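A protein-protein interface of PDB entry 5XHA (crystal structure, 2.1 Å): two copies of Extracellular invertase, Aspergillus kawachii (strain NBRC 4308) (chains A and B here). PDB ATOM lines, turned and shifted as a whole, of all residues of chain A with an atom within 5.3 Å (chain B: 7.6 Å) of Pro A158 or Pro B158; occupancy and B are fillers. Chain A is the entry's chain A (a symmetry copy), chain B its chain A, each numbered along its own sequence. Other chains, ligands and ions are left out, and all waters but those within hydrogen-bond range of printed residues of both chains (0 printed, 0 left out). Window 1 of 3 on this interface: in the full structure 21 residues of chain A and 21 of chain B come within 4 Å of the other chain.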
ATOM      1  N   ARG A 131      -4.396  19.901  30.347  1.00  0.00           N
ATOM      2  CA  ARG A 131      -5.197  21.068  30.041  1.00  0.00           C
ATOM      3  C   ARG A 131      -6.635  20.889  30.575  1.00  0.00           C
ATOM      4  O   ARG A 131      -7.226  19.812  30.440  1.00  0.00           O
ATOM      5  CB  ARG A 131      -5.182  21.297  28.521  1.00  0.00           C
ATOM      6  CG  ARG A 131      -5.915  22.546  28.044  1.00  0.00           C
ATOM      7  CD  ARG A 131      -5.061  23.808  28.141  1.00  0.00           C
ATOM      8  NE  ARG A 131      -5.820  24.972  27.668  1.00  0.00           N
ATOM      9  CZ  ARG A 131      -5.970  25.320  26.396  1.00  0.00           C
ATOM     10  NH1 ARG A 131      -5.405  24.601  25.435  1.00  0.00           N
ATOM     11  NH2 ARG A 131      -6.702  26.386  26.072  1.00  0.00           N
ATOM     12  N   GLU A 134      -8.299  21.638  36.014  1.00  0.00           N
ATOM     13  CA  GLU A 134      -8.878  22.479  37.059  1.00  0.00           C
ATOM     14  C   GLU A 134      -9.592  23.720  36.485  1.00  0.00           C
ATOM     15  O   GLU A 134      -9.009  24.522  35.744  1.00  0.00           O
ATOM     16  CB  GLU A 134      -7.799  22.890  38.053  1.00  0.00           C
ATOM     17  CG  GLU A 134      -7.130  21.716  38.745  1.00  0.00           C
ATOM     18  CD  GLU A 134      -5.859  22.112  39.457  1.00  0.00           C
ATOM     19  OE1 GLU A 134      -5.004  22.772  38.805  1.00  0.00           O
ATOM     20  OE2 GLU A 134      -5.716  21.756  40.655  1.00  0.00           O
ATOM     21  N   THR A 135     -10.874  23.852  36.800  1.00  0.00           N
ATOM     22  CA  THR A 135     -11.639  25.063  36.479  1.00  0.00           C
ATOM     23  C   THR A 135     -12.261  25.555  37.766  1.00  0.00           C
ATOM     24  O   THR A 135     -12.191  24.869  38.781  1.00  0.00           O
ATOM     25  CB  THR A 135     -12.753  24.792  35.468  1.00  0.00           C
ATOM     26  OG1 THR A 135     -13.639  23.794  35.995  1.00  0.00           O
ATOM     27  CG2 THR A 135     -12.175  24.318  34.137  1.00  0.00           C
ATOM     28  N   GLN A 136     -12.850  26.747  37.746  1.00  0.00           N
ATOM     29  CA  GLN A 136     -13.481  27.274  38.939  1.00  0.00           C
ATOM     30  C   GLN A 136     -14.956  27.480  38.620  1.00  0.00           C
ATOM     31  O   GLN A 136     -15.291  28.170  37.656  1.00  0.00           O
ATOM     32  CB  GLN A 136     -12.821  28.593  39.392  1.00  0.00           C
ATOM     33  CG  GLN A 136     -11.315  28.680  39.131  1.00  0.00           C
ATOM     34  CD  GLN A 136     -10.542  27.573  39.796  1.00  0.00           C
ATOM     35  OE1 GLN A 136     -10.917  27.090  40.877  1.00  0.00           O
ATOM     36  NE2 GLN A 136      -9.447  27.154  39.160  1.00  0.00           N
ATOM     37  N   PRO A 155     -17.946  26.396  34.102  1.00  0.00           N
ATOM     38  CA  PRO A 155     -17.177  27.167  35.054  1.00  0.00           C
ATOM     39  C   PRO A 155     -17.146  28.643  34.700  1.00  0.00           C
ATOM     40  O   PRO A 155     -17.171  28.997  33.514  1.00  0.00           O
ATOM     41  CB  PRO A 155     -15.760  26.578  34.945  1.00  0.00           C
ATOM     42  CG  PRO A 155     -15.726  25.894  33.630  1.00  0.00           C
ATOM     43  CD  PRO A 155     -17.129  25.391  33.400  1.00  0.00           C
ATOM     44  N   VAL A 156     -17.076  29.480  35.734  1.00  0.00           N
ATOM     45  CA  VAL A 156     -16.980  30.919  35.557  1.00  0.00           C
ATOM     46  C   VAL A 156     -15.541  31.358  35.285  1.00  0.00           C
ATOM     47  O   VAL A 156     -15.315  32.414  34.689  1.00  0.00           O
ATOM     48  CB  VAL A 156     -17.582  31.692  36.744  1.00  0.00           C
ATOM     49  CG1 VAL A 156     -19.072  31.397  36.830  1.00  0.00           C
ATOM     50  CG2 VAL A 156     -16.881  31.376  38.052  1.00  0.00           C
ATOM     51  N   ILE A 157     -14.582  30.528  35.690  1.00  0.00           N
ATOM     52  CA  ILE A 157     -13.185  30.690  35.289  1.00  0.00           C
ATOM     53  C   ILE A 157     -12.716  29.371  34.650  1.00  0.00           C
ATOM     54  O   ILE A 157     -12.247  28.483  35.350  1.00  0.00           O
ATOM     55  CB  ILE A 157     -12.273  31.083  36.469  1.00  0.00           C
ATOM     56  CG1 ILE A 157     -12.789  32.354  37.144  1.00  0.00           C
ATOM     57  CG2 ILE A 157     -10.846  31.289  35.979  1.00  0.00           C
ATOM     58  CD1 ILE A 157     -12.027  32.748  38.390  1.00  0.00           C
ATOM     59  N   PRO A 158     -12.880  29.235  33.321  1.00  0.00           N
ATOM     60  CA  PRO A 158     -12.632  27.955  32.658  1.00  0.00           C
ATOM     61  C   PRO A 158     -11.159  27.587  32.388  1.00  0.00           C
ATOM     62  O   PRO A 158     -10.885  26.685  31.623  1.00  0.00           O
ATOM     63  CB  PRO A 158     -13.412  28.086  31.349  1.00  0.00           C
ATOM     64  CG  PRO A 158     -13.515  29.554  31.097  1.00  0.00           C
ATOM     65  CD  PRO A 158     -13.580  30.190  32.440  1.00  0.00           C
ATOM     66  N   GLY A 159     -10.225  28.241  33.041  1.00  0.00           N
ATOM     67  CA  GLY A 159      -8.829  27.846  32.943  1.00  0.00           C
ATOM     68  C   GLY A 159      -7.953  29.047  33.192  1.00  0.00           C
ATOM     69  O   GLY A 159      -8.469  30.149  33.387  1.00  0.00           O
ATOM     70  N   PRO A 160      -6.630  28.832  33.202  1.00  0.00           N
ATOM     71  CA  PRO A 160      -5.657  29.880  33.465  1.00  0.00           C
ATOM     72  C   PRO A 160      -5.534  30.848  32.288  1.00  0.00           C
ATOM     73  O   PRO A 160      -6.070  30.586  31.229  1.00  0.00           O
ATOM     74  CB  PRO A 160      -4.348  29.107  33.680  1.00  0.00           C
ATOM     75  CG  PRO A 160      -4.546  27.794  33.018  1.00  0.00           C
ATOM     76  CD  PRO A 160      -6.004  27.512  32.999  1.00  0.00           C
ATOM     77  N   SER B 117     -17.592  20.752  21.284  1.00  0.00           N
ATOM     78  CA  SER B 117     -18.005  19.877  22.365  1.00  0.00           C
ATOM     79  C   SER B 117     -19.061  20.598  23.231  1.00  0.00           C
ATOM     80  O   SER B 117     -18.770  21.665  23.779  1.00  0.00           O
ATOM     81  CB  SER B 117     -16.788  19.509  23.206  1.00  0.00           C
ATOM     82  OG  SER B 117     -15.888  20.602  23.348  1.00  0.00           O
ATOM     83  N   ARG B 131     -23.535  29.740  29.965  1.00  0.00           N
ATOM     84  CA  ARG B 131     -22.090  29.817  29.992  1.00  0.00           C
ATOM     85  C   ARG B 131     -21.473  28.412  29.813  1.00  0.00           C
ATOM     86  O   ARG B 131     -21.945  27.437  30.408  1.00  0.00           O
ATOM     87  CB  ARG B 131     -21.651  30.463  31.315  1.00  0.00           C
ATOM     88  CG  ARG B 131     -20.149  30.694  31.460  1.00  0.00           C
ATOM     89  CD  ARG B 131     -19.681  31.984  30.790  1.00  0.00           C
ATOM     90  NE  ARG B 131     -18.233  32.148  30.965  1.00  0.00           N
ATOM     91  CZ  ARG B 131     -17.646  32.642  32.049  1.00  0.00           C
ATOM     92  NH1 ARG B 131     -18.376  33.043  33.081  1.00  0.00           N
ATOM     93  NH2 ARG B 131     -16.317  32.728  32.115  1.00  0.00           N
ATOM     94  N   GLY B 132     -20.451  28.299  28.963  1.00  0.00           N
ATOM     95  CA  GLY B 132     -19.772  27.011  28.748  1.00  0.00           C
ATOM     96  C   GLY B 132     -20.556  25.932  28.005  1.00  0.00           C
ATOM     97  O   GLY B 132     -20.133  24.764  27.971  1.00  0.00           O
ATOM     98  N   SER B 133     -21.680  26.286  27.386  1.00  0.00           N
ATOM     99  CA  SER B 133     -22.437  25.284  26.649  1.00  0.00           C
ATOM    100  C   SER B 133     -21.671  24.776  25.439  1.00  0.00           C
ATOM    101  O   SER B 133     -21.787  23.592  25.095  1.00  0.00           O
ATOM    102  CB  SER B 133     -23.851  25.755  26.280  1.00  0.00           C
ATOM    103  OG  SER B 133     -23.852  26.999  25.678  1.00  0.00           O
ATOM    104  N   GLU B 134     -20.858  25.641  24.827  1.00  0.00           N
ATOM    105  CA  GLU B 134     -20.037  25.264  23.678  1.00  0.00           C
ATOM    106  C   GLU B 134     -18.538  25.538  23.912  1.00  0.00           C
ATOM    107  O   GLU B 134     -18.122  26.662  24.221  1.00  0.00           O
ATOM    108  CB  GLU B 134     -20.528  25.987  22.430  1.00  0.00           C
ATOM    109  CG  GLU B 134     -21.969  25.671  22.072  1.00  0.00           C
ATOM    110  CD  GLU B 134     -22.537  26.632  21.055  1.00  0.00           C
ATOM    111  OE1 GLU B 134     -22.410  27.867  21.283  1.00  0.00           O
ATOM    112  OE2 GLU B 134     -23.113  26.154  20.045  1.00  0.00           O
ATOM    113  N   THR B 135     -17.730  24.492  23.803  1.00  0.00           N
ATOM    114  CA  THR B 135     -16.268  24.624  23.822  1.00  0.00           C
ATOM    115  C   THR B 135     -15.740  23.951  22.576  1.00  0.00           C
ATOM    116  O   THR B 135     -16.499  23.307  21.859  1.00  0.00           O
ATOM    117  CB  THR B 135     -15.644  23.953  25.045  1.00  0.00           C
ATOM    118  OG1 THR B 135     -15.996  22.562  25.054  1.00  0.00           O
ATOM    119  CG2 THR B 135     -16.124  24.615  26.334  1.00  0.00           C
ATOM    120  N   GLN B 136     -14.450  24.111  22.292  1.00  0.00           N
ATOM    121  CA  GLN B 136     -13.873  23.481  21.123  1.00  0.00           C
ATOM    122  C   GLN B 136     -12.781  22.536  21.607  1.00  0.00           C
ATOM    123  O   GLN B 136     -11.870  22.956  22.323  1.00  0.00           O
ATOM    124  CB  GLN B 136     -13.307  24.526  20.139  1.00  0.00           C
ATOM    125  CG  GLN B 136     -14.084  25.843  20.085  1.00  0.00           C
ATOM    126  CD  GLN B 136     -15.530  25.653  19.712  1.00  0.00           C
ATOM    127  OE1 GLN B 136     -15.878  24.742  18.943  1.00  0.00           O
ATOM    128  NE2 GLN B 136     -16.395  26.514  20.248  1.00  0.00           N
ATOM    129  N   SER B 137     -12.879  21.270  21.196  1.00  0.00           N
ATOM    130  CA  SER B 137     -12.023  20.193  21.665  1.00  0.00           C
ATOM    131  C   SER B 137     -11.329  19.491  20.493  1.00  0.00           C
ATOM    132  O   SER B 137     -11.758  19.613  19.333  1.00  0.00           O
ATOM    133  CB  SER B 137     -12.867  19.189  22.462  1.00  0.00           C
ATOM    134  OG  SER B 137     -13.322  19.752  23.689  1.00  0.00           O
ATOM    135  N   GLY B 154      -9.000  18.733  28.561  1.00  0.00           N
ATOM    136  CA  GLY B 154     -10.073  19.681  28.330  1.00  0.00           C
ATOM    137  C   GLY B 154     -10.056  20.330  26.955  1.00  0.00           C
ATOM    138  O   GLY B 154      -9.151  20.104  26.157  1.00  0.00           O
ATOM    139  N   PRO B 155     -11.065  21.162  26.677  1.00  0.00           N
ATOM    140  CA  PRO B 155     -11.083  21.841  25.399  1.00  0.00           C
ATOM    141  C   PRO B 155      -9.878  22.747  25.219  1.00  0.00           C
ATOM    142  O   PRO B 155      -9.376  23.313  26.198  1.00  0.00           O
ATOM    143  CB  PRO B 155     -12.365  22.688  25.450  1.00  0.00           C
ATOM    144  CG  PRO B 155     -12.692  22.808  26.892  1.00  0.00           C
ATOM    145  CD  PRO B 155     -12.216  21.525  27.523  1.00  0.00           C
ATOM    146  N   VAL B 156      -9.443  22.883  23.967  1.00  0.00           N
ATOM    147  CA  VAL B 156      -8.338  23.761  23.624  1.00  0.00           C
ATOM    148  C   VAL B 156      -8.798  25.211  23.473  1.00  0.00           C
ATOM    149  O   VAL B 156      -7.996  26.137  23.624  1.00  0.00           O
ATOM    150  CB  VAL B 156      -7.584  23.283  22.371  1.00  0.00           C
ATOM    151  CG1 VAL B 156      -6.947  21.929  22.654  1.00  0.00           C
ATOM    152  CG2 VAL B 156      -8.477  23.226  21.147  1.00  0.00           C
ATOM    153  N   ILE B 157     -10.090  25.399  23.211  1.00  0.00           N
ATOM    154  CA  ILE B 157     -10.720  26.718  23.280  1.00  0.00           C
ATOM    155  C   ILE B 157     -11.921  26.622  24.237  1.00  0.00           C
ATOM    156  O   ILE B 157     -13.021  26.295  23.809  1.00  0.00           O
ATOM    157  CB  ILE B 157     -11.159  27.236  21.896  1.00  0.00           C
ATOM    158  CG1 ILE B 157      -9.973  27.257  20.932  1.00  0.00           C
ATOM    159  CG2 ILE B 157     -11.756  28.631  22.026  1.00  0.00           C
ATOM    160  CD1 ILE B 157     -10.334  27.635  19.512  1.00  0.00           C
ATOM    161  N   PRO B 158     -11.697  26.876  25.540  1.00  0.00           N
ATOM    162  CA  PRO B 158     -12.733  26.636  26.543  1.00  0.00           C
ATOM    163  C   PRO B 158     -13.847  27.695  26.658  1.00  0.00           C
ATOM    164  O   PRO B 158     -14.583  27.706  27.623  1.00  0.00           O
ATOM    165  CB  PRO B 158     -11.937  26.535  27.845  1.00  0.00           C
ATOM    166  CG  PRO B 158     -10.678  27.297  27.597  1.00  0.00           C
ATOM    167  CD  PRO B 158     -10.376  27.118  26.152  1.00  0.00           C
ATOM    168  N   GLY B 159     -14.001  28.545  25.668  1.00  0.00           N
ATOM    169  CA  GLY B 159     -15.121  29.472  25.646  1.00  0.00           C
ATOM    170  C   GLY B 159     -14.740  30.696  24.853  1.00  0.00           C
ATOM    171  O   GLY B 159     -13.602  30.792  24.389  1.00  0.00           O
ATOM    172  N   PRO B 160     -15.694  31.621  24.684  1.00  0.00           N
ATOM    173  CA  PRO B 160     -15.494  32.838  23.913  1.00  0.00           C
ATOM    174  C   PRO B 160     -14.598  33.834  24.649  1.00  0.00           C
ATOM    175  O   PRO B 160     -14.299  33.638  25.811  1.00  0.00           O
ATOM    176  CB  PRO B 160     -16.914  33.395  23.746  1.00  0.00           C
ATOM    177  CG  PRO B 160     -17.713  32.786  24.840  1.00  0.00           C
ATOM    178  CD  PRO B 160     -17.068  31.501  25.211  1.00  0.00           C
ATOM    179  N   PHE B 169     -21.426  29.926  19.566  1.00  0.00           N
ATOM    180  CA  PHE B 169     -19.960  29.820  19.537  1.00  0.00           C
ATOM    181  C   PHE B 169     -19.556  28.399  19.130  1.00  0.00           C
ATOM    182  O   PHE B 169     -19.154  27.590  19.958  1.00  0.00           O
ATOM    183  CB  PHE B 169     -19.399  30.197  20.906  1.00  0.00           C
ATOM    184  CG  PHE B 169     -17.892  30.315  20.957  1.00  0.00           C
ATOM    185  CD1 PHE B 169     -17.249  31.354  20.330  1.00  0.00           C
ATOM    186  CD2 PHE B 169     -17.137  29.418  21.701  1.00  0.00           C
ATOM    187  CE1 PHE B 169     -15.869  31.472  20.380  1.00  0.00           C
ATOM    188  CE2 PHE B 169     -15.754  29.530  21.770  1.00  0.00           C
ATOM    189  CZ  PHE B 169     -15.119  30.561  21.102  1.00  0.00           C
ATOM    190  N   GLN B 217      -2.686  23.350  20.559  1.00  0.00           N
ATOM    191  CA  GLN B 217      -3.203  23.428  21.910  1.00  0.00           C
ATOM    192  C   GLN B 217      -3.802  24.807  22.209  1.00  0.00           C
ATOM    193  O   GLN B 217      -4.839  24.920  22.881  1.00  0.00           O
ATOM    194  CB  GLN B 217      -2.032  23.116  22.837  1.00  0.00           C
ATOM    195  CG  GLN B 217      -2.386  22.887  24.269  1.00  0.00           C
ATOM    196  CD  GLN B 217      -3.301  21.701  24.461  1.00  0.00           C
ATOM    197  OE1 GLN B 217      -3.207  20.675  23.767  1.00  0.00           O
ATOM    198  NE2 GLN B 217      -4.212  21.851  25.385  1.00  0.00           N
ATOM    199  N   TYR B 218      -3.146  25.853  21.692  1.00  0.00           N
ATOM    200  CA  TYR B 218      -3.517  27.225  21.951  1.00  0.00           C
ATOM    201  C   TYR B 218      -3.843  27.976  20.667  1.00  0.00           C
ATOM    202  O   TYR B 218      -3.169  27.817  19.636  1.00  0.00           O
ATOM    203  CB  TYR B 218      -2.414  27.950  22.743  1.00  0.00           C
ATOM    204  CG  TYR B 218      -2.188  27.352  24.097  1.00  0.00           C
ATOM    205  CD1 TYR B 218      -3.142  27.509  25.104  1.00  0.00           C
ATOM    206  CD2 TYR B 218      -1.036  26.610  24.381  1.00  0.00           C
ATOM    207  CE1 TYR B 218      -2.968  26.945  26.350  1.00  0.00           C
ATOM    208  CE2 TYR B 218      -0.854  26.032  25.638  1.00  0.00           C
ATOM    209  CZ  TYR B 218      -1.825  26.213  26.618  1.00  0.00           C
ATOM    210  OH  TYR B 218      -1.682  25.665  27.869  1.00  0.00           O
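Printed residues of chain B within 4 Å of Pro A155: Arg B131 (3.96 Å). Of the printed residues of chain B, Val A156 touches Arg B131 (2.8 Å). Of chain B, only Arg B131 and Pro B158 come within 4 Å of Pro A158. Of the printed residues of chain A, Arg B131 touches Pro A155 (3.96 Å), Val A156 (2.8 Å) and Pro A158 (3.7 Å). Of chain A, only Arg A131 and Pro A158 come within 4 Å of Pro B158. Of the printed residues of chain A, Tyr B218 touches Arg A131 (3.4 Å). The nearest residue of chain B that does not touch Pro A158 is Gly B159 (5.5 Å). The nearest printed residue of chain A that does not touch Arg B131 is Ile A157 (4.5 Å).
NH2 of Arg B131 sits at hydrogen-bond distance from O of Val A156. The guanidinium group (NH1) of Arg A131 is in hydrogen-bond range of the backbone carbonyl oxygen (O) of Gln B217. N of Gly B154 sits at hydrogen-bond distance from O of Arg A131 (2.8 Å). The backbone carbonyl oxygen of Val B156 is in hydrogen-bond range of the guanidinium group of Arg A131 (2.8 Å).
Among the printed residues, pairs that only touch across the chains: Arg A131 with Pro B155 (3.96 Å), Arg A131 with Pro B158 (3.7 Å), Arg A131 with Tyr B218 (3.4 Å), Pro A155 with Arg B131 (3.96 Å), Pro A158 with Arg B131 (3.7 Å) and Pro A158 with Pro B158 (3.9 Å).
Arg A131 touches Pro B155, and with the chains exchanged Pro A155 touches Arg B131. Arg A131 touches Val B156, and with the chains exchanged Val A156 touches Arg B131. Arg A131 touches Pro B158, and with the chains exchanged Pro A158 touches Arg B131. Pro B158 touches its own counterpart, Pro A158. Of the 10 pairs that touch across the chains among the printed residues, 7 have their exchanged pair printed and touching as well.
The backbone NH (N) of Val B156 lies within hydrogen-bond range of the backbone carbonyl oxygen (O) of Gln B136, at 2.9 Å. O of Gln A136 is in hydrogen-bond range of N of Val A156.
Of the 18 printed residues of chain B, 7 touch a printed residue of chain A. Hydrophobic or aromatic side chains of chain B that line the printed part of chain A: Val B156, Pro B158 and Tyr B218.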
